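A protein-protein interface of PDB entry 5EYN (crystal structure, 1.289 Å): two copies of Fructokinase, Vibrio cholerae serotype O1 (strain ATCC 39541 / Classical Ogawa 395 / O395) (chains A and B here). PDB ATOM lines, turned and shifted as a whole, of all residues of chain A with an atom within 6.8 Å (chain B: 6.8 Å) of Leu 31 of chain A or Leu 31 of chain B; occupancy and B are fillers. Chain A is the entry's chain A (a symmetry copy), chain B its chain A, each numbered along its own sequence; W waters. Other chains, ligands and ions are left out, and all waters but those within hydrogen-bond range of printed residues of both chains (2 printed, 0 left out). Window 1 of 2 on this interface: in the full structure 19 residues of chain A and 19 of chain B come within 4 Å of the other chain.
The backbone NH of Tyr 39 of chain B sits at hydrogen-bond distance from the backbone carbonyl oxygen of Tyr 39 of chain A, 2.8 Å away.
The backbone carbonyl oxygen of Val 101 of chain B sits at hydrogen-bond distance from the backbone NH of Leu 31 of chain B (2.7 Å). O of Leu 31 of chain B is in hydrogen-bond range of N of Val 103 of chain B (2.9 Å). The backbone carbonyl oxygen (O) of Thr 100 of chain B sits at hydrogen-bond distance from the backbone NH (N) of Met 116 of chain B, at 2.9 Å. The backbone NH of Leu 31 of chain A is in hydrogen-bond range of the backbone carbonyl oxygen of Val 101 of chain A. O of Leu 31 of chain A sits at hydrogen-bond distance from N of Val 103 of chain A (2.9 Å). The backbone NH (N) of Met 116 of chain A is in hydrogen-bond range of the backbone carbonyl oxygen (O) of Thr 100 of chain A, at 2.9 Å.
Leu 31 of chain B touches Leu 31 of chain A (CD1 to CD1, 3.8 Å). Tyr 39 of chain A touches Lys 41 of chain B. Tyr 39 of chain A touches Phe 72 of chain B. Lys 41 of chain A touches Tyr 39 of chain B (CD to OH, 3.6 Å). CE1 of Phe 72 of chain A touches OH of Tyr 39 of chain B, at 3.3 Å. CZ of Phe 72 of chain A touches CG2 of Val 102 of chain B (3.5 Å). Met 116 of chain B touches Phe 72 of chain A. Thr 100 of chain A touches Met 116 of chain B. CE of Met 116 of chain A touches CD2 of Phe 72 of chain B, at 3.8 Å. OG1 of Thr 100 of chain B touches CE of Met 116 of chain A, 3.5 Å away.
Of chain B, only Leu 31 comes within 4 Å of Leu 31 of chain A. Leu 31 of chain B touches one residue of chain A. Printed residues of chain A within 4 Å of Phe 72 of chain B: Tyr 39 (3.3 Å), Val 102 (3.5 Å) and Met 116 (3.8 Å). Printed residues of chain A within 4 Å of Met 116 of chain B: Phe 72 and Thr 100. Printed residues of chain B within 4 Å of Tyr 39 of chain A: Tyr 39, Lys 41 and Phe 72. Of the printed residues of chain B, Val 102 of chain A touches Phe 72 (3.5 Å). Leu 40 of chain B touches none of the printed residues of chain A. Val 101 of chain B touches none of the printed residues of chain A. The nearest residue of chain A that does not touch Leu 31 of chain B is Tyr 39 of chain A (4.1 Å).
Of the 16 printed residues of chain B, 7 touch a printed residue of chain A. Of the 16 printed residues of chain A, 7 touch a printed residue of chain B. Printed residues of chain A that touch a printed residue of chain B: Leu 31, Tyr 39, Lys 41, Phe 72, Thr 100, Val 102 and Met 116. Hydrophobic or aromatic side chains of chain A within 4 Å of the printed part of chain B: Leu 31, Tyr 39, Phe 72, Val 102 and Met 116. Among the printed residues, no Asp or Glu carboxylate lies within 4 Å of a Lys or Arg side-chain nitrogen of the other chain.
Leu 31 of chain A touches its own counterpart, Leu 31 of chain B. Tyr 39 of chain A touches its own counterpart, Tyr 39 of chain B. Tyr 39 of chain A touches Phe 72 of chain B, and with the chains exchanged Phe 72 of chain A touches Tyr 39 of chain B. Thr 100 of chain A touches Met 116 of chain B, and with the chains exchanged Met 116 of chain A touches Thr 100 of chain B.
Water W1 bridges N of Phe 72 of chain B and SD of Met 116 of chain A. Water W2 bridges the backbone NH (N) of Phe 72 of chain A (3.0 Å) and the side-chain sulfur (SD) of Met 116 of chain B (3.3 Å).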
ATOM      1  N   VAL A  29      18.469  25.024  -4.922  1.00  0.00           N
ATOM      2  CA  VAL A  29      18.132  24.392  -3.656  1.00  0.00           C
ATOM      3  C   VAL A  29      18.173  22.885  -3.837  1.00  0.00           C
ATOM      4  O   VAL A  29      17.438  22.319  -4.655  1.00  0.00           O
ATOM      5  CB  VAL A  29      16.766  24.868  -3.099  1.00  0.00           C
ATOM      6  CG1 VAL A  29      16.321  23.998  -1.943  1.00  0.00           C
ATOM      7  CG2 VAL A  29      16.856  26.324  -2.665  1.00  0.00           C
ATOM      8  N   ASP A  30      19.073  22.255  -3.081  1.00  0.00           N
ATOM      9  CA  ASP A  30      19.178  20.809  -3.020  1.00  0.00           C
ATOM     10  C   ASP A  30      18.302  20.310  -1.867  1.00  0.00           C
ATOM     11  O   ASP A  30      18.490  20.685  -0.698  1.00  0.00           O
ATOM     12  CB  ASP A  30      20.622  20.365  -2.753  1.00  0.00           C
ATOM     13  CG  ASP A  30      21.561  20.567  -3.936  1.00  0.00           C
ATOM     14  OD1 ASP A  30      21.117  20.509  -5.101  1.00  0.00           O
ATOM     15  OD2 ASP A  30      22.778  20.706  -3.671  1.00  0.00           O
ATOM     16  N   LEU A  31      17.349  19.456  -2.191  1.00  0.00           N
ATOM     17  CA  LEU A  31      16.482  18.830  -1.203  1.00  0.00           C
ATOM     18  C   LEU A  31      17.094  17.480  -0.863  1.00  0.00           C
ATOM     19  O   LEU A  31      17.126  16.570  -1.682  1.00  0.00           O
ATOM     20  CB  LEU A  31      15.079  18.687  -1.799  1.00  0.00           C
ATOM     21  CG  LEU A  31      14.374  19.999  -2.121  1.00  0.00           C
ATOM     22  CD1 LEU A  31      13.122  19.740  -2.948  1.00  0.00           C
ATOM     23  CD2 LEU A  31      14.042  20.787  -0.870  1.00  0.00           C
ATOM     24  N   ILE A  32      17.610  17.374   0.354  1.00  0.00           N
ATOM     25  CA  ILE A  32      18.421  16.233   0.741  1.00  0.00           C
ATOM     26  C   ILE A  32      17.698  15.460   1.836  1.00  0.00           C
ATOM     27  O   ILE A  32      17.389  16.022   2.889  1.00  0.00           O
ATOM     28  CB  ILE A  32      19.817  16.672   1.218  1.00  0.00           C
ATOM     29  CG1 ILE A  32      20.501  17.438   0.073  1.00  0.00           C
ATOM     30  CG2 ILE A  32      20.643  15.467   1.654  1.00  0.00           C
ATOM     31  CD1 ILE A  32      21.957  17.798   0.346  1.00  0.00           C
ATOM     32  N   PRO A  33      17.421  14.175   1.587  1.00  0.00           N
ATOM     33  CA  PRO A  33      16.703  13.379   2.590  1.00  0.00           C
ATOM     34  C   PRO A  33      17.358  13.433   3.958  1.00  0.00           C
ATOM     35  O   PRO A  33      18.579  13.332   4.081  1.00  0.00           O
ATOM     36  CB  PRO A  33      16.787  11.962   2.030  1.00  0.00           C
ATOM     37  CG  PRO A  33      16.876  12.170   0.538  1.00  0.00           C
ATOM     38  CD  PRO A  33      17.738  13.377   0.390  1.00  0.00           C
ATOM     39  N   TYR A  39      12.904  16.464   3.819  1.00  0.00           N
ATOM     40  CA  TYR A  39      14.098  16.943   3.143  1.00  0.00           C
ATOM     41  C   TYR A  39      14.701  18.100   3.920  1.00  0.00           C
ATOM     42  O   TYR A  39      13.977  18.986   4.376  1.00  0.00           O
ATOM     43  CB  TYR A  39      13.765  17.473   1.749  1.00  0.00           C
ATOM     44  CG  TYR A  39      13.361  16.428   0.749  1.00  0.00           C
ATOM     45  CD1 TYR A  39      14.277  15.516   0.258  1.00  0.00           C
ATOM     46  CD2 TYR A  39      12.060  16.370   0.279  1.00  0.00           C
ATOM     47  CE1 TYR A  39      13.900  14.561  -0.659  1.00  0.00           C
ATOM     48  CE2 TYR A  39      11.686  15.431  -0.630  1.00  0.00           C
ATOM     49  CZ  TYR A  39      12.601  14.521  -1.088  1.00  0.00           C
ATOM     50  OH  TYR A  39      12.213  13.570  -2.002  1.00  0.00           O
ATOM     51  N   LEU A  40      16.028  18.115   4.015  1.00  0.00           N
ATOM     52  CA  LEU A  40      16.752  19.317   4.365  1.00  0.00           C
ATOM     53  C   LEU A  40      16.693  20.249   3.184  1.00  0.00           C
ATOM     54  O   LEU A  40      16.843  19.817   2.045  1.00  0.00           O
ATOM     55  CB  LEU A  40      18.213  18.990   4.620  1.00  0.00           C
ATOM     56  CG  LEU A  40      18.555  18.385   5.974  1.00  0.00           C
ATOM     57  CD1 LEU A  40      19.948  17.793   5.927  1.00  0.00           C
ATOM     58  CD2 LEU A  40      18.443  19.450   7.058  1.00  0.00           C
ATOM     59  N   LYS A  41      16.498  21.529   3.463  1.00  0.00           N
ATOM     60  CA  LYS A  41      16.546  22.572   2.452  1.00  0.00           C
ATOM     61  C   LYS A  41      17.983  23.083   2.424  1.00  0.00           C
ATOM     62  O   LYS A  41      18.370  23.900   3.246  1.00  0.00           O
ATOM     63  CB  LYS A  41      15.600  23.705   2.816  1.00  0.00           C
ATOM     64  CG  LYS A  41      15.576  24.823   1.800  1.00  0.00           C
ATOM     65  CD  LYS A  41      14.736  25.999   2.244  1.00  0.00           C
ATOM     66  CE  LYS A  41      15.484  26.923   3.148  1.00  0.00           C
ATOM     67  NZ  LYS A  41      14.560  27.968   3.648  1.00  0.00           N
ATOM     68  N   CYS A  42      18.789  22.588   1.497  1.00  0.00           N
ATOM     69  CA  CYS A  42      20.222  22.893   1.482  1.00  0.00           C
ATOM     70  C   CYS A  42      20.584  23.806   0.300  1.00  0.00           C
ATOM     71  O   CYS A  42      20.199  23.554  -0.859  1.00  0.00           O
ATOM     72  CB  CYS A  42      21.034  21.614   1.350  1.00  0.00           C
ATOM     73  SG  CYS A  42      20.924  20.574   2.803  1.00  0.00           S
ATOM     74  N   PHE A  72      13.031  30.282  -3.004  1.00  0.00           N
ATOM     75  CA  PHE A  72      14.295  29.580  -3.141  1.00  0.00           C
ATOM     76  C   PHE A  72      15.380  30.512  -3.695  1.00  0.00           C
ATOM     77  O   PHE A  72      16.543  30.471  -3.259  1.00  0.00           O
ATOM     78  CB  PHE A  72      14.152  28.340  -4.015  1.00  0.00           C
ATOM     79  CG  PHE A  72      13.492  27.175  -3.325  1.00  0.00           C
ATOM     80  CD1 PHE A  72      13.038  27.258  -2.011  1.00  0.00           C
ATOM     81  CD2 PHE A  72      13.348  25.983  -3.996  1.00  0.00           C
ATOM     82  CE1 PHE A  72      12.445  26.168  -1.406  1.00  0.00           C
ATOM     83  CE2 PHE A  72      12.752  24.897  -3.396  1.00  0.00           C
ATOM     84  CZ  PHE A  72      12.294  24.990  -2.103  1.00  0.00           C
ATOM     85  N   THR A 100      15.609  23.527  -8.538  1.00  0.00           N
ATOM     86  CA  THR A 100      15.256  22.720  -7.383  1.00  0.00           C
ATOM     87  C   THR A 100      15.625  21.293  -7.694  1.00  0.00           C
ATOM     88  O   THR A 100      15.129  20.717  -8.653  1.00  0.00           O
ATOM     89  CB  THR A 100      13.759  22.822  -7.101  1.00  0.00           C
ATOM     90  OG1 THR A 100      13.418  24.186  -6.901  1.00  0.00           O
ATOM     91  CG2 THR A 100      13.377  22.042  -5.862  1.00  0.00           C
ATOM     92  N   VAL A 101      16.506  20.726  -6.873  1.00  0.00           N
ATOM     93  CA  VAL A 101      17.088  19.442  -7.162  1.00  0.00           C
ATOM     94  C   VAL A 101      16.813  18.496  -6.001  1.00  0.00           C
ATOM     95  O   VAL A 101      17.013  18.840  -4.836  1.00  0.00           O
ATOM     96  CB  VAL A 101      18.600  19.590  -7.376  1.00  0.00           C
ATOM     97  CG1 VAL A 101      19.276  18.242  -7.502  1.00  0.00           C
ATOM     98  CG2 VAL A 101      18.872  20.439  -8.606  1.00  0.00           C
ATOM     99  N   VAL A 102      16.329  17.304  -6.312  1.00  0.00           N
ATOM    100  CA  VAL A 102      16.093  16.275  -5.299  1.00  0.00           C
ATOM    101  C   VAL A 102      17.277  15.314  -5.295  1.00  0.00           C
ATOM    102  O   VAL A 102      17.678  14.792  -6.332  1.00  0.00           O
ATOM    103  CB  VAL A 102      14.785  15.517  -5.571  1.00  0.00           C
ATOM    104  CG1 VAL A 102      14.563  14.427  -4.539  1.00  0.00           C
ATOM    105  CG2 VAL A 102      13.619  16.489  -5.584  1.00  0.00           C
ATOM    106  N   VAL A 103      17.870  15.123  -4.125  1.00  0.00           N
ATOM    107  CA  VAL A 103      19.046  14.265  -3.989  1.00  0.00           C
ATOM    108  C   VAL A 103      18.694  12.865  -3.473  1.00  0.00           C
ATOM    109  O   VAL A 103      17.910  12.727  -2.534  1.00  0.00           O
ATOM    110  CB  VAL A 103      20.073  14.912  -3.039  1.00  0.00           C
ATOM    111  CG1 VAL A 103      21.324  14.054  -2.894  1.00  0.00           C
ATOM    112  CG2 VAL A 103      20.439  16.320  -3.508  1.00  0.00           C
ATOM    113  N   ASP A 104      19.284  11.841  -4.088  1.00  0.00           N
ATOM    114  CA  ASP A 104      19.204  10.450  -3.609  1.00  0.00           C
ATOM    115  C   ASP A 104      20.566  10.068  -3.038  1.00  0.00           C
ATOM    116  O   ASP A 104      21.540   9.937  -3.776  1.00  0.00           O
ATOM    117  CB  ASP A 104      18.845   9.534  -4.785  1.00  0.00           C
ATOM    118  CG  ASP A 104      18.676   8.076  -4.383  1.00  0.00           C
ATOM    119  OD1 ASP A 104      18.267   7.271  -5.253  1.00  0.00           O
ATOM    120  OD2 ASP A 104      18.934   7.730  -3.217  1.00  0.00           O
ATOM    121  N   MET A 116      14.159  19.217 -10.911  1.00  0.00           N
ATOM    122  CA  MET A 116      12.725  19.425 -11.020  1.00  0.00           C
ATOM    123  C   MET A 116      12.329  20.623 -11.869  1.00  0.00           C
ATOM    124  O   MET A 116      11.199  20.676 -12.359  1.00  0.00           O
ATOM    125  CB  MET A 116      12.076  19.542  -9.644  1.00  0.00           C
ATOM    126  CG  MET A 116      12.242  18.318  -8.780  1.00  0.00           C
ATOM    127  SD  MET A 116      11.673  16.793  -9.525  1.00  0.00           S
ATOM    128  CE  MET A 116       9.913  17.132  -9.659  1.00  0.00           C
ATOM    129  N   VAL B  29       3.665  17.242  -5.204  1.00  0.00           N
ATOM    130  CA  VAL B  29       4.332  17.155  -3.915  1.00  0.00           C
ATOM    131  C   VAL B  29       4.349  18.534  -3.280  1.00  0.00           C
ATOM    132  O   VAL B  29       4.907  19.487  -3.837  1.00  0.00           O
ATOM    133  CB  VAL B  29       5.755  16.552  -4.020  1.00  0.00           C
ATOM    134  CG1 VAL B  29       6.517  16.732  -2.724  1.00  0.00           C
ATOM    135  CG2 VAL B  29       5.674  15.077  -4.389  1.00  0.00           C
ATOM    136  N   ASP B  30       3.696  18.626  -2.121  1.00  0.00           N
ATOM    137  CA  ASP B  30       3.704  19.824  -1.304  1.00  0.00           C
ATOM    138  C   ASP B  30       4.858  19.717  -0.302  1.00  0.00           C
ATOM    139  O   ASP B  30       4.926  18.783   0.515  1.00  0.00           O
ATOM    140  CB  ASP B  30       2.396  19.971  -0.516  1.00  0.00           C
ATOM    141  CG  ASP B  30       1.193  20.345  -1.375  1.00  0.00           C
ATOM    142  OD1 ASP B  30       1.354  21.021  -2.411  1.00  0.00           O
ATOM    143  OD2 ASP B  30       0.067  20.008  -0.941  1.00  0.00           O
ATOM    144  N   LEU B  31       5.762  20.677  -0.355  1.00  0.00           N
ATOM    145  CA  LEU B  31       6.876  20.763   0.578  1.00  0.00           C
ATOM    146  C   LEU B  31       6.452  21.702   1.696  1.00  0.00           C
ATOM    147  O   LEU B  31       6.289  22.900   1.495  1.00  0.00           O
ATOM    148  CB  LEU B  31       8.106  21.284  -0.170  1.00  0.00           C
ATOM    149  CG  LEU B  31       8.627  20.373  -1.276  1.00  0.00           C
ATOM    150  CD1 LEU B  31       9.664  21.103  -2.119  1.00  0.00           C
ATOM    151  CD2 LEU B  31       9.191  19.078  -0.726  1.00  0.00           C
ATOM    152  N   ILE B  32       6.245  21.133   2.875  1.00  0.00           N
ATOM    153  CA  ILE B  32       5.625  21.857   3.973  1.00  0.00           C
ATOM    154  C   ILE B  32       6.635  22.004   5.103  1.00  0.00           C
ATOM    155  O   ILE B  32       7.145  21.003   5.610  1.00  0.00           O
ATOM    156  CB  ILE B  32       4.354  21.144   4.468  1.00  0.00           C
ATOM    157  CG1 ILE B  32       3.371  21.032   3.292  1.00  0.00           C
ATOM    158  CG2 ILE B  32       3.736  21.896   5.641  1.00  0.00           C
ATOM    159  CD1 ILE B  32       2.000  20.487   3.674  1.00  0.00           C
ATOM    160  N   PRO B  33       6.930  23.249   5.492  1.00  0.00           N
ATOM    161  CA  PRO B  33       7.914  23.462   6.560  1.00  0.00           C
ATOM    162  C   PRO B  33       7.597  22.670   7.815  1.00  0.00           C
ATOM    163  O   PRO B  33       6.449  22.613   8.256  1.00  0.00           O
ATOM    164  CB  PRO B  33       7.795  24.957   6.845  1.00  0.00           C
ATOM    165  CG  PRO B  33       7.344  25.539   5.528  1.00  0.00           C
ATOM    166  CD  PRO B  33       6.394  24.525   4.989  1.00  0.00           C
ATOM    167  N   TYR B  39      11.683  20.444   5.096  1.00  0.00           N
ATOM    168  CA  TYR B  39      10.335  20.302   4.573  1.00  0.00           C
ATOM    169  C   TYR B  39       9.857  18.873   4.762  1.00  0.00           C
ATOM    170  O   TYR B  39      10.607  17.929   4.512  1.00  0.00           O
ATOM    171  CB  TYR B  39      10.295  20.587   3.072  1.00  0.00           C
ATOM    172  CG  TYR B  39      10.521  22.021   2.689  1.00  0.00           C
ATOM    173  CD1 TYR B  39       9.578  22.992   2.967  1.00  0.00           C
ATOM    174  CD2 TYR B  39      11.676  22.398   2.025  1.00  0.00           C
ATOM    175  CE1 TYR B  39       9.791  24.306   2.613  1.00  0.00           C
ATOM    176  CE2 TYR B  39      11.887  23.693   1.669  1.00  0.00           C
ATOM    177  CZ  TYR B  39      10.952  24.646   1.974  1.00  0.00           C
ATOM    178  OH  TYR B  39      11.176  25.955   1.617  1.00  0.00           O
ATOM    179  N   LEU B  40       8.591  18.724   5.145  1.00  0.00           N
ATOM    180  CA  LEU B  40       7.892  17.468   4.986  1.00  0.00           C
ATOM    181  C   LEU B  40       7.610  17.281   3.519  1.00  0.00           C
ATOM    182  O   LEU B  40       7.225  18.226   2.837  1.00  0.00           O
ATOM    183  CB  LEU B  40       6.556  17.520   5.708  1.00  0.00           C
ATOM    184  CG  LEU B  40       6.584  17.319   7.216  1.00  0.00           C
ATOM    185  CD1 LEU B  40       5.261  17.758   7.809  1.00  0.00           C
ATOM    186  CD2 LEU B  40       6.877  15.859   7.537  1.00  0.00           C
ATOM    187  N   LYS B  41       7.780  16.055   3.046  1.00  0.00           N
ATOM    188  CA  LYS B  41       7.426  15.680   1.687  1.00  0.00           C
ATOM    189  C   LYS B  41       5.992  15.161   1.739  1.00  0.00           C
ATOM    190  O   LYS B  41       5.757  14.015   2.089  1.00  0.00           O
ATOM    191  CB  LYS B  41       8.354  14.586   1.183  1.00  0.00           C
ATOM    192  CG  LYS B  41       8.065  14.153  -0.235  1.00  0.00           C
ATOM    193  CD  LYS B  41       8.906  12.974  -0.670  1.00  0.00           C
ATOM    194  CE  LYS B  41       8.332  11.670  -0.223  1.00  0.00           C
ATOM    195  NZ  LYS B  41       9.277  10.581  -0.564  1.00  0.00           N
ATOM    196  N   CYS B  42       5.025  16.008   1.419  1.00  0.00           N
ATOM    197  CA  CYS B  42       3.613  15.660   1.586  1.00  0.00           C
ATOM    198  C   CYS B  42       2.923  15.462   0.227  1.00  0.00           C
ATOM    199  O   CYS B  42       3.040  16.299  -0.690  1.00  0.00           O
ATOM    200  CB  CYS B  42       2.878  16.768   2.326  1.00  0.00           C
ATOM    201  SG  CYS B  42       3.396  16.919   4.033  1.00  0.00           S
ATOM    202  N   PHE B  72       9.042  12.119  -7.602  1.00  0.00           N
ATOM    203  CA  PHE B  72       7.830  12.707  -7.057  1.00  0.00           C
ATOM    204  C   PHE B  72       6.586  12.122  -7.738  1.00  0.00           C
ATOM    205  O   PHE B  72       5.563  11.856  -7.083  1.00  0.00           O
ATOM    206  CB  PHE B  72       7.845  14.225  -7.175  1.00  0.00           C
ATOM    207  CG  PHE B  72       8.725  14.912  -6.162  1.00  0.00           C
ATOM    208  CD1 PHE B  72       9.469  14.196  -5.228  1.00  0.00           C
ATOM    209  CD2 PHE B  72       8.785  16.285  -6.137  1.00  0.00           C
ATOM    210  CE1 PHE B  72      10.258  14.857  -4.308  1.00  0.00           C
ATOM    211  CE2 PHE B  72       9.577  16.945  -5.225  1.00  0.00           C
ATOM    212  CZ  PHE B  72      10.318  16.232  -4.313  1.00  0.00           C
ATOM    213  N   THR B 100       5.688  20.569  -8.092  1.00  0.00           N
ATOM    214  CA  THR B 100       6.355  20.690  -6.807  1.00  0.00           C
ATOM    215  C   THR B 100       6.018  22.046  -6.244  1.00  0.00           C
ATOM    216  O   THR B 100       6.312  23.065  -6.857  1.00  0.00           O
ATOM    217  CB  THR B 100       7.866  20.557  -6.980  1.00  0.00           C
ATOM    218  OG1 THR B 100       8.154  19.310  -7.595  1.00  0.00           O
ATOM    219  CG2 THR B 100       8.579  20.613  -5.646  1.00  0.00           C
ATOM    220  N   VAL B 101       5.395  22.051  -5.068  1.00  0.00           N
ATOM    221  CA  VAL B 101       4.847  23.260  -4.510  1.00  0.00           C
ATOM    222  C   VAL B 101       5.450  23.490  -3.131  1.00  0.00           C
ATOM    223  O   VAL B 101       5.507  22.585  -2.300  1.00  0.00           O
ATOM    224  CB  VAL B 101       3.321  23.143  -4.408  1.00  0.00           C
ATOM    225  CG1 VAL B 101       2.725  24.316  -3.660  1.00  0.00           C
ATOM    226  CG2 VAL B 101       2.711  23.030  -5.795  1.00  0.00           C
ATOM    227  N   VAL B 102       5.925  24.702  -2.890  1.00  0.00           N
ATOM    228  CA  VAL B 102       6.459  25.078  -1.581  1.00  0.00           C
ATOM    229  C   VAL B 102       5.376  25.819  -0.805  1.00  0.00           C
ATOM    230  O   VAL B 102       4.778  26.772  -1.299  1.00  0.00           O
ATOM    231  CB  VAL B 102       7.714  25.952  -1.723  1.00  0.00           C
ATOM    232  CG1 VAL B 102       8.245  26.369  -0.364  1.00  0.00           C
ATOM    233  CG2 VAL B 102       8.777  25.204  -2.507  1.00  0.00           C
ATOM    234  N   VAL B 103       5.089  25.342   0.398  1.00  0.00           N
ATOM    235  CA  VAL B 103       4.037  25.929   1.227  1.00  0.00           C
ATOM    236  C   VAL B 103       4.592  26.885   2.289  1.00  0.00           C
ATOM    237  O   VAL B 103       5.582  26.572   2.951  1.00  0.00           O
ATOM    238  CB  VAL B 103       3.222  24.820   1.920  1.00  0.00           C
ATOM    239  CG1 VAL B 103       2.100  25.396   2.774  1.00  0.00           C
ATOM    240  CG2 VAL B 103       2.664  23.832   0.896  1.00  0.00           C
ATOM    241  N   ASP B 104       3.943  28.038   2.447  1.00  0.00           N
ATOM    242  CA  ASP B 104       4.226  28.986   3.537  1.00  0.00           C
ATOM    243  C   ASP B 104       3.065  28.930   4.525  1.00  0.00           C
ATOM    244  O   ASP B 104       1.955  29.357   4.212  1.00  0.00           O
ATOM    245  CB  ASP B 104       4.358  30.398   2.953  1.00  0.00           C
ATOM    246  CG  ASP B 104       4.713  31.451   3.994  1.00  0.00           C
ATOM    247  OD1 ASP B 104       4.959  32.612   3.593  1.00  0.00           O
ATOM    248  OD2 ASP B 104       4.759  31.130   5.195  1.00  0.00           O
ATOM    249  N   MET B 116       6.820  25.571  -8.177  1.00  0.00           N
ATOM    250  CA  MET B 116       8.173  25.544  -8.711  1.00  0.00           C
ATOM    251  C   MET B 116       8.277  24.982 -10.120  1.00  0.00           C
ATOM    252  O   MET B 116       9.254  25.263 -10.818  1.00  0.00           O
ATOM    253  CB  MET B 116       9.117  24.780  -7.788  1.00  0.00           C
ATOM    254  CG  MET B 116       9.240  25.373  -6.407  1.00  0.00           C
ATOM    255  SD  MET B 116       9.718  27.097  -6.373  1.00  0.00           S
ATOM    256  CE  MET B 116      11.371  26.993  -7.072  1.00  0.00           C
HETATM  257  O   HOH W   1      11.375  13.898  -8.064  1.00  0.00           O
HETATM  258  O   HOH W   2      10.542  28.844  -3.751  1.00  0.00           O
